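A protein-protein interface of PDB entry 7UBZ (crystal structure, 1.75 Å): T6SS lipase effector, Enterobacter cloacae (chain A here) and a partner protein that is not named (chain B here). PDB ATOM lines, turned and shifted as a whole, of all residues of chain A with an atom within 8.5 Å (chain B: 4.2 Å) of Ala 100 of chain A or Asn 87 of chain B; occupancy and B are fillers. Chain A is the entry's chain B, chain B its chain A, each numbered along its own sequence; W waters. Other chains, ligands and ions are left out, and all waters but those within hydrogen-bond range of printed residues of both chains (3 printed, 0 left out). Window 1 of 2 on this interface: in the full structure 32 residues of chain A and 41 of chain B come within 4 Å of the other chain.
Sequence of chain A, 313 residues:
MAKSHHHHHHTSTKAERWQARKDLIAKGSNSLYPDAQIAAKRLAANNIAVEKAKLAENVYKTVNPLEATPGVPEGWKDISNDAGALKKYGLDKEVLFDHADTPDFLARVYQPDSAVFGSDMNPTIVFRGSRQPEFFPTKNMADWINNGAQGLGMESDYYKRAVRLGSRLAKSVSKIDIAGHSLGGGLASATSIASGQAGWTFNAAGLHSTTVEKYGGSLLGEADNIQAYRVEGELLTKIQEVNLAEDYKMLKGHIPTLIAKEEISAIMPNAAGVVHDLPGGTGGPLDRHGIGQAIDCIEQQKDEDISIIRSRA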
ATOM      1  N   GLU A  94      28.681   4.641  11.998  1.00  0.00           N
ATOM      2  CA  GLU A  94      29.090   3.337  12.491  1.00  0.00           C
ATOM      3  C   GLU A  94      30.303   3.449  13.400  1.00  0.00           C
ATOM      4  O   GLU A  94      30.378   2.761  14.413  1.00  0.00           O
ATOM      5  CB  GLU A  94      29.407   2.421  11.298  1.00  0.00           C
ATOM      6  CG  GLU A  94      29.519   0.907  11.690  1.00  0.00           C
ATOM      7  CD  GLU A  94      30.911   0.524  12.211  1.00  0.00           C
ATOM      8  OE1 GLU A  94      31.910   1.187  11.888  1.00  0.00           O
ATOM      9  OE2 GLU A  94      30.999  -0.423  13.006  1.00  0.00           O
ATOM     10  N   PHE A  97      30.265   4.386  17.744  1.00  0.00           N
ATOM     11  CA  PHE A  97      29.946   3.636  18.954  1.00  0.00           C
ATOM     12  C   PHE A  97      30.215   2.154  18.711  1.00  0.00           C
ATOM     13  O   PHE A  97      30.376   1.724  17.574  1.00  0.00           O
ATOM     14  CB  PHE A  97      28.494   3.842  19.458  1.00  0.00           C
ATOM     15  CG  PHE A  97      27.353   3.606  18.453  1.00  0.00           C
ATOM     16  CD1 PHE A  97      27.170   4.403  17.330  1.00  0.00           C
ATOM     17  CD2 PHE A  97      26.409   2.597  18.708  1.00  0.00           C
ATOM     18  CE1 PHE A  97      26.060   4.232  16.471  1.00  0.00           C
ATOM     19  CE2 PHE A  97      25.315   2.398  17.851  1.00  0.00           C
ATOM     20  CZ  PHE A  97      25.151   3.215  16.713  1.00  0.00           C
ATOM     21  N   ASP A  98      30.352   1.414  19.802  1.00  0.00           N
ATOM     22  CA  ASP A  98      30.417  -0.051  19.840  1.00  0.00           C
ATOM     23  C   ASP A  98      29.054  -0.630  19.465  1.00  0.00           C
ATOM     24  O   ASP A  98      28.024  -0.004  19.742  1.00  0.00           O
ATOM     25  CB  ASP A  98      30.736  -0.509  21.272  1.00  0.00           C
ATOM     26  CG  ASP A  98      32.197  -0.289  21.688  1.00  0.00           C
ATOM     27  OD1 ASP A  98      33.099  -0.178  20.842  1.00  0.00           O
ATOM     28  OD2 ASP A  98      32.426  -0.224  22.914  1.00  0.00           O
ATOM     29  N   HIS A  99      29.029  -1.873  18.946  1.00  0.00           N
ATOM     30  CA  HIS A  99      27.753  -2.440  18.480  1.00  0.00           C
ATOM     31  C   HIS A  99      27.407  -3.817  19.024  1.00  0.00           C
ATOM     32  O   HIS A  99      26.299  -4.278  18.762  1.00  0.00           O
ATOM     33  CB  HIS A  99      27.717  -2.503  16.932  1.00  0.00           C
ATOM     34  CG  HIS A  99      27.993  -1.176  16.292  1.00  0.00           C
ATOM     35  ND1 HIS A  99      27.004  -0.229  16.171  1.00  0.00           N
ATOM     36  CD2 HIS A  99      29.110  -0.628  15.747  1.00  0.00           C
ATOM     37  CE1 HIS A  99      27.496   0.863  15.608  1.00  0.00           C
ATOM     38  NE2 HIS A  99      28.772   0.653  15.339  1.00  0.00           N
ATOM     39  N   ALA A 100      28.289  -4.471  19.780  1.00  0.00           N
ATOM     40  CA  ALA A 100      27.927  -5.806  20.275  1.00  0.00           C
ATOM     41  C   ALA A 100      26.885  -5.762  21.388  1.00  0.00           C
ATOM     42  O   ALA A 100      26.051  -6.671  21.489  1.00  0.00           O
ATOM     43  CB  ALA A 100      29.192  -6.557  20.733  1.00  0.00           C
ATOM     44  N   ASP A 101      26.894  -4.733  22.230  1.00  0.00           N
ATOM     45  CA  ASP A 101      26.015  -4.644  23.386  1.00  0.00           C
ATOM     46  C   ASP A 101      25.640  -3.178  23.565  1.00  0.00           C
ATOM     47  O   ASP A 101      25.955  -2.332  22.719  1.00  0.00           O
ATOM     48  CB  ASP A 101      26.742  -5.240  24.600  1.00  0.00           C
ATOM     49  CG  ASP A 101      25.800  -5.708  25.728  1.00  0.00           C
ATOM     50  OD1 ASP A 101      24.573  -5.444  25.727  1.00  0.00           O
ATOM     51  OD2 ASP A 101      26.340  -6.369  26.643  1.00  0.00           O
ATOM     52  N   THR A 102      24.989  -2.872  24.679  1.00  0.00           N
ATOM     53  CA  THR A 102      24.872  -1.485  25.119  1.00  0.00           C
ATOM     54  C   THR A 102      26.231  -0.806  24.991  1.00  0.00           C
ATOM     55  O   THR A 102      27.232  -1.356  25.467  1.00  0.00           O
ATOM     56  CB  THR A 102      24.406  -1.461  26.570  1.00  0.00           C
ATOM     57  OG1 THR A 102      23.093  -2.029  26.621  1.00  0.00           O
ATOM     58  CG2 THR A 102      24.380  -0.025  27.090  1.00  0.00           C
ATOM     59  N   PRO A 103      26.326   0.347  24.325  1.00  0.00           N
ATOM     60  CA  PRO A 103      27.661   0.854  23.982  1.00  0.00           C
ATOM     61  C   PRO A 103      28.506   1.156  25.209  1.00  0.00           C
ATOM     62  O   PRO A 103      28.025   1.664  26.219  1.00  0.00           O
ATOM     63  CB  PRO A 103      27.383   2.102  23.131  1.00  0.00           C
ATOM     64  CG  PRO A 103      25.983   2.405  23.256  1.00  0.00           C
ATOM     65  CD  PRO A 103      25.252   1.201  23.823  1.00  0.00           C
ATOM     66  N   ASP A 104      29.751   0.719  25.142  1.00  0.00           N
ATOM     67  CA  ASP A 104      30.762   1.108  26.104  1.00  0.00           C
ATOM     68  C   ASP A 104      31.518   2.310  25.537  1.00  0.00           C
ATOM     69  O   ASP A 104      31.511   3.401  26.120  1.00  0.00           O
ATOM     70  CB  ASP A 104      31.675  -0.088  26.372  1.00  0.00           C
ATOM     71  CG  ASP A 104      32.767   0.218  27.363  1.00  0.00           C
ATOM     72  OD1 ASP A 104      32.585   1.139  28.188  1.00  0.00           O
ATOM     73  OD2 ASP A 104      33.817  -0.461  27.291  1.00  0.00           O
ATOM     74  N   TRP A 144      22.717 -11.954  28.529  1.00  0.00           N
ATOM     75  CA  TRP A 144      23.177 -13.064  27.707  1.00  0.00           C
ATOM     76  C   TRP A 144      24.273 -12.637  26.740  1.00  0.00           C
ATOM     77  O   TRP A 144      25.144 -13.452  26.394  1.00  0.00           O
ATOM     78  CB  TRP A 144      21.998 -13.688  26.953  1.00  0.00           C
ATOM     79  CG  TRP A 144      21.251 -12.772  26.005  1.00  0.00           C
ATOM     80  CD1 TRP A 144      20.161 -11.995  26.292  1.00  0.00           C
ATOM     81  CD2 TRP A 144      21.529 -12.578  24.615  1.00  0.00           C
ATOM     82  NE1 TRP A 144      19.746 -11.331  25.164  1.00  0.00           N
ATOM     83  CE2 TRP A 144      20.570 -11.675  24.119  1.00  0.00           C
ATOM     84  CE3 TRP A 144      22.490 -13.101  23.731  1.00  0.00           C
ATOM     85  CZ2 TRP A 144      20.548 -11.267  22.782  1.00  0.00           C
ATOM     86  CZ3 TRP A 144      22.445 -12.722  22.389  1.00  0.00           C
ATOM     87  CH2 TRP A 144      21.497 -11.799  21.936  1.00  0.00           C
ATOM     88  N   ILE A 145      24.272 -11.371  26.306  1.00  0.00           N
ATOM     89  CA  ILE A 145      25.317 -10.932  25.383  1.00  0.00           C
ATOM     90  C   ILE A 145      26.686 -11.030  26.041  1.00  0.00           C
ATOM     91  O   ILE A 145      27.637 -11.569  25.463  1.00  0.00           O
ATOM     92  CB  ILE A 145      25.032  -9.505  24.872  1.00  0.00           C
ATOM     93  CG1 ILE A 145      23.928  -9.573  23.824  1.00  0.00           C
ATOM     94  CG2 ILE A 145      26.294  -8.908  24.223  1.00  0.00           C
ATOM     95  CD1 ILE A 145      24.460 -10.076  22.490  1.00  0.00           C
ATOM     96  N   ASN A 146      26.805 -10.525  27.276  1.00  0.00           N
ATOM     97  CA  ASN A 146      28.089 -10.571  27.961  1.00  0.00           C
ATOM     98  C   ASN A 146      28.584 -12.016  28.134  1.00  0.00           C
ATOM     99  O   ASN A 146      29.767 -12.294  27.918  1.00  0.00           O
ATOM    100  CB  ASN A 146      27.970  -9.841  29.305  1.00  0.00           C
ATOM    101  CG  ASN A 146      29.313  -9.570  29.950  1.00  0.00           C
ATOM    102  OD1 ASN A 146      29.566  -9.995  31.071  1.00  0.00           O
ATOM    103  ND2 ASN A 146      30.173  -8.841  29.249  1.00  0.00           N
ATOM    104  N   GLY A 148      27.873 -14.417  25.955  1.00  0.00           N
ATOM    105  CA  GLY A 148      28.322 -14.782  24.616  1.00  0.00           C
ATOM    106  C   GLY A 148      29.667 -14.172  24.280  1.00  0.00           C
ATOM    107  O   GLY A 148      30.548 -14.838  23.737  1.00  0.00           O
ATOM    108  N   ALA A 149      29.858 -12.907  24.639  1.00  0.00           N
ATOM    109  CA  ALA A 149      31.136 -12.261  24.347  1.00  0.00           C
ATOM    110  C   ALA A 149      32.301 -12.985  25.039  1.00  0.00           C
ATOM    111  O   ALA A 149      33.378 -13.171  24.441  1.00  0.00           O
ATOM    112  CB  ALA A 149      31.064 -10.783  24.743  1.00  0.00           C
ATOM    113  N   LEU A 152      33.119 -16.336  23.262  1.00  0.00           N
ATOM    114  CA  LEU A 152      33.641 -16.036  21.940  1.00  0.00           C
ATOM    115  C   LEU A 152      34.995 -15.355  21.975  1.00  0.00           C
ATOM    116  O   LEU A 152      35.539 -15.078  20.918  1.00  0.00           O
ATOM    117  CB  LEU A 152      32.641 -15.178  21.146  1.00  0.00           C
ATOM    118  CG  LEU A 152      31.255 -15.736  20.820  1.00  0.00           C
ATOM    119  CD1 LEU A 152      30.511 -14.784  19.888  1.00  0.00           C
ATOM    120  CD2 LEU A 152      31.462 -16.983  20.089  1.00  0.00           C
ATOM    121  N   MET A 154      35.864 -12.404  22.965  1.00  0.00           N
ATOM    122  CA  MET A 154      35.807 -11.019  22.544  1.00  0.00           C
ATOM    123  C   MET A 154      36.752 -10.153  23.363  1.00  0.00           C
ATOM    124  O   MET A 154      36.808 -10.260  24.590  1.00  0.00           O
ATOM    125  CB  MET A 154      34.372 -10.535  22.649  1.00  0.00           C
ATOM    126  CG  MET A 154      33.857 -10.294  21.271  1.00  0.00           C
ATOM    127  SD  MET A 154      32.132  -9.872  21.103  1.00  0.00           S
ATOM    128  CE  MET A 154      31.616 -11.496  20.644  1.00  0.00           C
ATOM    129  N   SER A 156      36.689  -6.796  23.836  1.00  0.00           N
ATOM    130  CA  SER A 156      35.897  -5.829  24.626  1.00  0.00           C
ATOM    131  C   SER A 156      36.739  -4.656  25.145  1.00  0.00           C
ATOM    132  O   SER A 156      36.758  -4.351  26.344  1.00  0.00           O
ATOM    133  CB  SER A 156      35.181  -6.531  25.784  1.00  0.00           C
ATOM    134  OG  SER A 156      33.860  -6.894  25.416  1.00  0.00           O
ATOM    135  N   ARG A 161      38.136   1.439  19.583  1.00  0.00           N
ATOM    136  CA  ARG A 161      37.413   2.399  18.755  1.00  0.00           C
ATOM    137  C   ARG A 161      37.825   3.839  19.040  1.00  0.00           C
ATOM    138  O   ARG A 161      37.706   4.686  18.156  1.00  0.00           O
ATOM    139  CB  ARG A 161      35.902   2.206  18.930  1.00  0.00           C
ATOM    140  CG  ARG A 161      35.438   1.032  18.056  1.00  0.00           C
ATOM    141  CD  ARG A 161      33.882   0.851  18.042  1.00  0.00           C
ATOM    142  NE  ARG A 161      33.536  -0.253  17.149  1.00  0.00           N
ATOM    143  CZ  ARG A 161      32.945  -0.122  15.964  1.00  0.00           C
ATOM    144  NH1 ARG A 161      32.492   1.048  15.541  1.00  0.00           N
ATOM    145  NH2 ARG A 161      32.823  -1.192  15.174  1.00  0.00           N
ATOM    146  N   PHE B  49      20.718 -15.965  17.371  1.00  0.00           N
ATOM    147  CA  PHE B  49      21.579 -15.641  18.515  1.00  0.00           C
ATOM    148  C   PHE B  49      21.506 -16.750  19.576  1.00  0.00           C
ATOM    149  O   PHE B  49      22.515 -17.101  20.192  1.00  0.00           O
ATOM    150  CB  PHE B  49      21.191 -14.282  19.131  1.00  0.00           C
ATOM    151  CG  PHE B  49      21.984 -13.105  18.575  1.00  0.00           C
ATOM    152  CD1 PHE B  49      23.360 -13.017  18.758  1.00  0.00           C
ATOM    153  CD2 PHE B  49      21.335 -12.114  17.877  1.00  0.00           C
ATOM    154  CE1 PHE B  49      24.074 -11.931  18.223  1.00  0.00           C
ATOM    155  CE2 PHE B  49      22.026 -10.993  17.319  1.00  0.00           C
ATOM    156  CZ  PHE B  49      23.417 -10.925  17.515  1.00  0.00           C
ATOM    157  N   ARG B  82      19.910  -5.891  15.439  1.00  0.00           N
ATOM    158  CA  ARG B  82      19.196  -5.643  16.689  1.00  0.00           C
ATOM    159  C   ARG B  82      18.857  -4.163  16.781  1.00  0.00           C
ATOM    160  O   ARG B  82      19.337  -3.353  15.978  1.00  0.00           O
ATOM    161  CB  ARG B  82      20.045  -6.080  17.876  1.00  0.00           C
ATOM    162  CG  ARG B  82      20.046  -7.626  18.038  1.00  0.00           C
ATOM    163  CD  ARG B  82      20.970  -8.027  19.186  1.00  0.00           C
ATOM    164  NE  ARG B  82      22.379  -7.829  18.829  1.00  0.00           N
ATOM    165  CZ  ARG B  82      23.345  -7.559  19.702  1.00  0.00           C
ATOM    166  NH1 ARG B  82      23.090  -7.397  20.996  1.00  0.00           N
ATOM    167  NH2 ARG B  82      24.601  -7.472  19.274  1.00  0.00           N
ATOM    168  N   GLY B  85      21.058   0.165  16.750  1.00  0.00           N
ATOM    169  CA  GLY B  85      22.355   0.039  16.097  1.00  0.00           C
ATOM    170  C   GLY B  85      23.181  -1.122  16.588  1.00  0.00           C
ATOM    171  O   GLY B  85      24.401  -1.141  16.359  1.00  0.00           O
ATOM    172  N   LYS B  86      22.573  -2.064  17.307  1.00  0.00           N
ATOM    173  CA  LYS B  86      23.294  -3.273  17.728  1.00  0.00           C
ATOM    174  C   LYS B  86      23.357  -4.288  16.601  1.00  0.00           C
ATOM    175  O   LYS B  86      22.507  -4.310  15.698  1.00  0.00           O
ATOM    176  CB  LYS B  86      22.642  -3.890  18.960  1.00  0.00           C
ATOM    177  CG  LYS B  86      22.828  -2.956  20.166  1.00  0.00           C
ATOM    178  CD  LYS B  86      22.073  -3.472  21.365  1.00  0.00           C
ATOM    179  CE  LYS B  86      22.067  -2.490  22.511  1.00  0.00           C
ATOM    180  NZ  LYS B  86      20.881  -2.739  23.393  1.00  0.00           N
ATOM    181  N   ASN B  87      24.407  -5.098  16.629  1.00  0.00           N
ATOM    182  CA  ASN B  87      24.765  -5.788  15.396  1.00  0.00           C
ATOM    183  C   ASN B  87      24.143  -7.179  15.269  1.00  0.00           C
ATOM    184  O   ASN B  87      23.494  -7.709  16.183  1.00  0.00           O
ATOM    185  CB  ASN B  87      26.291  -5.833  15.203  1.00  0.00           C
ATOM    186  CG  ASN B  87      27.052  -6.626  16.274  1.00  0.00           C
ATOM    187  OD1 ASN B  87      26.512  -7.374  17.078  1.00  0.00           O
ATOM    188  ND2 ASN B  87      28.367  -6.451  16.253  1.00  0.00           N
ATOM    189  N   SER B  88      24.272  -7.720  14.058  1.00  0.00           N
ATOM    190  CA  SER B  88      23.660  -8.998  13.682  1.00  0.00           C
ATOM    191  C   SER B  88      24.507 -10.164  14.148  1.00  0.00           C
ATOM    192  O   SER B  88      25.686  -9.991  14.481  1.00  0.00           O
ATOM    193  CB  SER B  88      23.550  -9.093  12.162  1.00  0.00           C
ATOM    194  OG  SER B  88      24.865  -9.116  11.580  1.00  0.00           O
ATOM    195  N   GLU B  91      27.910 -10.236  12.169  1.00  0.00           N
ATOM    196  CA  GLU B  91      28.876  -9.242  12.643  1.00  0.00           C
ATOM    197  C   GLU B  91      29.412  -9.599  14.012  1.00  0.00           C
ATOM    198  O   GLU B  91      30.613  -9.442  14.280  1.00  0.00           O
ATOM    199  CB  GLU B  91      28.255  -7.860  12.660  1.00  0.00           C
ATOM    200  CG  GLU B  91      27.820  -7.317  11.284  1.00  0.00           C
ATOM    201  CD  GLU B  91      26.865  -6.152  11.516  1.00  0.00           C
ATOM    202  OE1 GLU B  91      27.289  -4.978  11.311  1.00  0.00           O
ATOM    203  OE2 GLU B  91      25.684  -6.433  11.834  1.00  0.00           O
ATOM    204  N   PHE B  92      28.533 -10.094  14.880  1.00  0.00           N
ATOM    205  CA  PHE B  92      28.911 -10.432  16.246  1.00  0.00           C
ATOM    206  C   PHE B  92      29.988 -11.504  16.265  1.00  0.00           C
ATOM    207  O   PHE B  92      31.024 -11.347  16.940  1.00  0.00           O
ATOM    208  CB  PHE B  92      27.646 -10.884  16.976  1.00  0.00           C
ATOM    209  CG  PHE B  92      27.780 -11.081  18.472  1.00  0.00           C
ATOM    210  CD1 PHE B  92      27.718 -10.012  19.357  1.00  0.00           C
ATOM    211  CD2 PHE B  92      27.881 -12.367  18.980  1.00  0.00           C
ATOM    212  CE1 PHE B  92      27.801 -10.217  20.756  1.00  0.00           C
ATOM    213  CE2 PHE B  92      27.969 -12.588  20.385  1.00  0.00           C
ATOM    214  CZ  PHE B  92      27.937 -11.518  21.255  1.00  0.00           C
ATOM    215  N   MET B  95      33.754 -10.877  15.529  1.00  0.00           N
ATOM    216  CA  MET B  95      34.538 -10.253  16.601  1.00  0.00           C
ATOM    217  C   MET B  95      35.212 -11.319  17.474  1.00  0.00           C
ATOM    218  O   MET B  95      36.016 -10.984  18.360  1.00  0.00           O
ATOM    219  CB  MET B  95      33.517  -9.445  17.414  1.00  0.00           C
ATOM    220  CG  MET B  95      32.987  -8.313  16.600  1.00  0.00           C
ATOM    221  SD  MET B  95      31.915  -7.198  17.523  1.00  0.00           S
ATOM    222  CE  MET B  95      33.157  -6.181  18.349  1.00  0.00           C
HETATM  223  O   HOH W   1      21.285  -0.737  25.185  1.00  0.00           O
HETATM  224  O   HOH W   2      28.585  -2.260  12.944  1.00  0.00           O
HETATM  225  O   HOH W   3      22.220  -5.417  24.434  1.00  0.00           O
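Among the printed residues, merely in contact across the chains: His 99 of chain A with Lys 86 of chain B, Ile 145 of chain A with Arg 82 of chain B, Leu 152 of chain A with Phe 92 of chain B, Trp 144 of chain A with Phe 49 of chain B, His 99 of chain A with Arg 82 of chain B, Thr 102 of chain A with Lys 86 of chain B, Met 154 of chain A with Met 95 of chain B, Met 154 of chain A with Phe 92 of chain B, Ile 145 of chain A with Phe 92 of chain B, Asp 101 of chain A with Lys 86 of chain B, Ala 100 of chain A with Asn 87 of chain B, Ala 100 of chain A with Phe 92 of chain B and Phe 97 of chain A with Gly 85 of chain B.
The backbone carbonyl oxygen (O) of Gly 85 of chain B is in hydrogen-bond range of a ring nitrogen (ND1) of His 99 of chain A. N of Asn 87 of chain B sits at hydrogen-bond distance from O of His 99 of chain A. O of Ala 100 of chain A is in hydrogen-bond range of NH2 of Arg 82 of chain B (2.8 Å).
Water W1 lies within hydrogen-bond range of the side-chain hydroxyl of Thr 102 of chain A and the side-chain amino group of Lys 86 of chain B. Water W3 lies within hydrogen-bond range of OD1 of Asp 101 of chain A (2.7 Å) and NZ of Lys 86 of chain B (3.2 Å). Water W2 lies within hydrogen-bond range of OE2 of Glu 94 of chain A and OE1 of Glu 91 of chain B.
Ala 100 of chain A touches three residues of chain B. Asn 87 of chain B touches just these residues of chain A: His 99 (3.0 Å) and Ala 100 (3.8 Å). Ser 88 of chain B touches none of the printed residues of chain A. Printed residues of chain B within 4 Å of His 99 of chain A: Arg 82, Gly 85, Lys 86 and Asn 87. Of the printed residues of chain B, Phe 97 of chain A touches Gly 85 (3.9 Å). Printed residues of chain B within 4 Å of Asp 101 of chain A: Lys 86. Of the printed residues of chain B, Ile 145 of chain A touches Arg 82 and Phe 92. The nearest printed residue of chain B that does not touch Ala 100 of chain A is Met 95 of chain B (4.3 Å). The nearest residue of chain A that does not touch Asn 87 of chain B is Asp 101 of chain A (5.8 Å). The nearest printed residue of chain A that does not touch Met 95 of chain B is Ala 100 of chain A (4.3 Å).
NE of Arg 82 of chain B lies within hydrogen-bond range of O of Asn 87 of chain B, at 2.9 Å. O of Phe 97 of chain A is in hydrogen-bond range of NE2 of His 99 of chain A (3.0 Å). The backbone carbonyl oxygen (O) of Phe 97 of chain A sits at hydrogen-bond distance from the guanidinium group (NH1) of Arg 161 of chain A (3.0 Å). O of Ala 149 of chain A sits at hydrogen-bond distance from N of Met 154 of chain A (3.0 Å). The backbone carbonyl oxygen (O) of Glu 94 of chain A lies within hydrogen-bond range of a ring nitrogen (NE2) of His 99 of chain A (2.8 Å).
Hydrophobic or aromatic side chains of chain B that line the printed part of chain A: Phe 49, Phe 92 and Met 95. Along chain B the printed residues that touch a printed residue of chain A span positions 49 to 95. Printed residues of chain A that touch a printed residue of chain B: Phe 97, His 99, Ala 100, Asp 101, Thr 102, Trp 144, Ile 145, Leu 152 and Met 154. Hydrophobic or aromatic side chains of chain A that line the printed part of chain B: Phe 97, His 99, Ala 100, Trp 144, Ile 145, Leu 152 and Met 154. Among the printed residues, 16 pairs touch across the chains.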
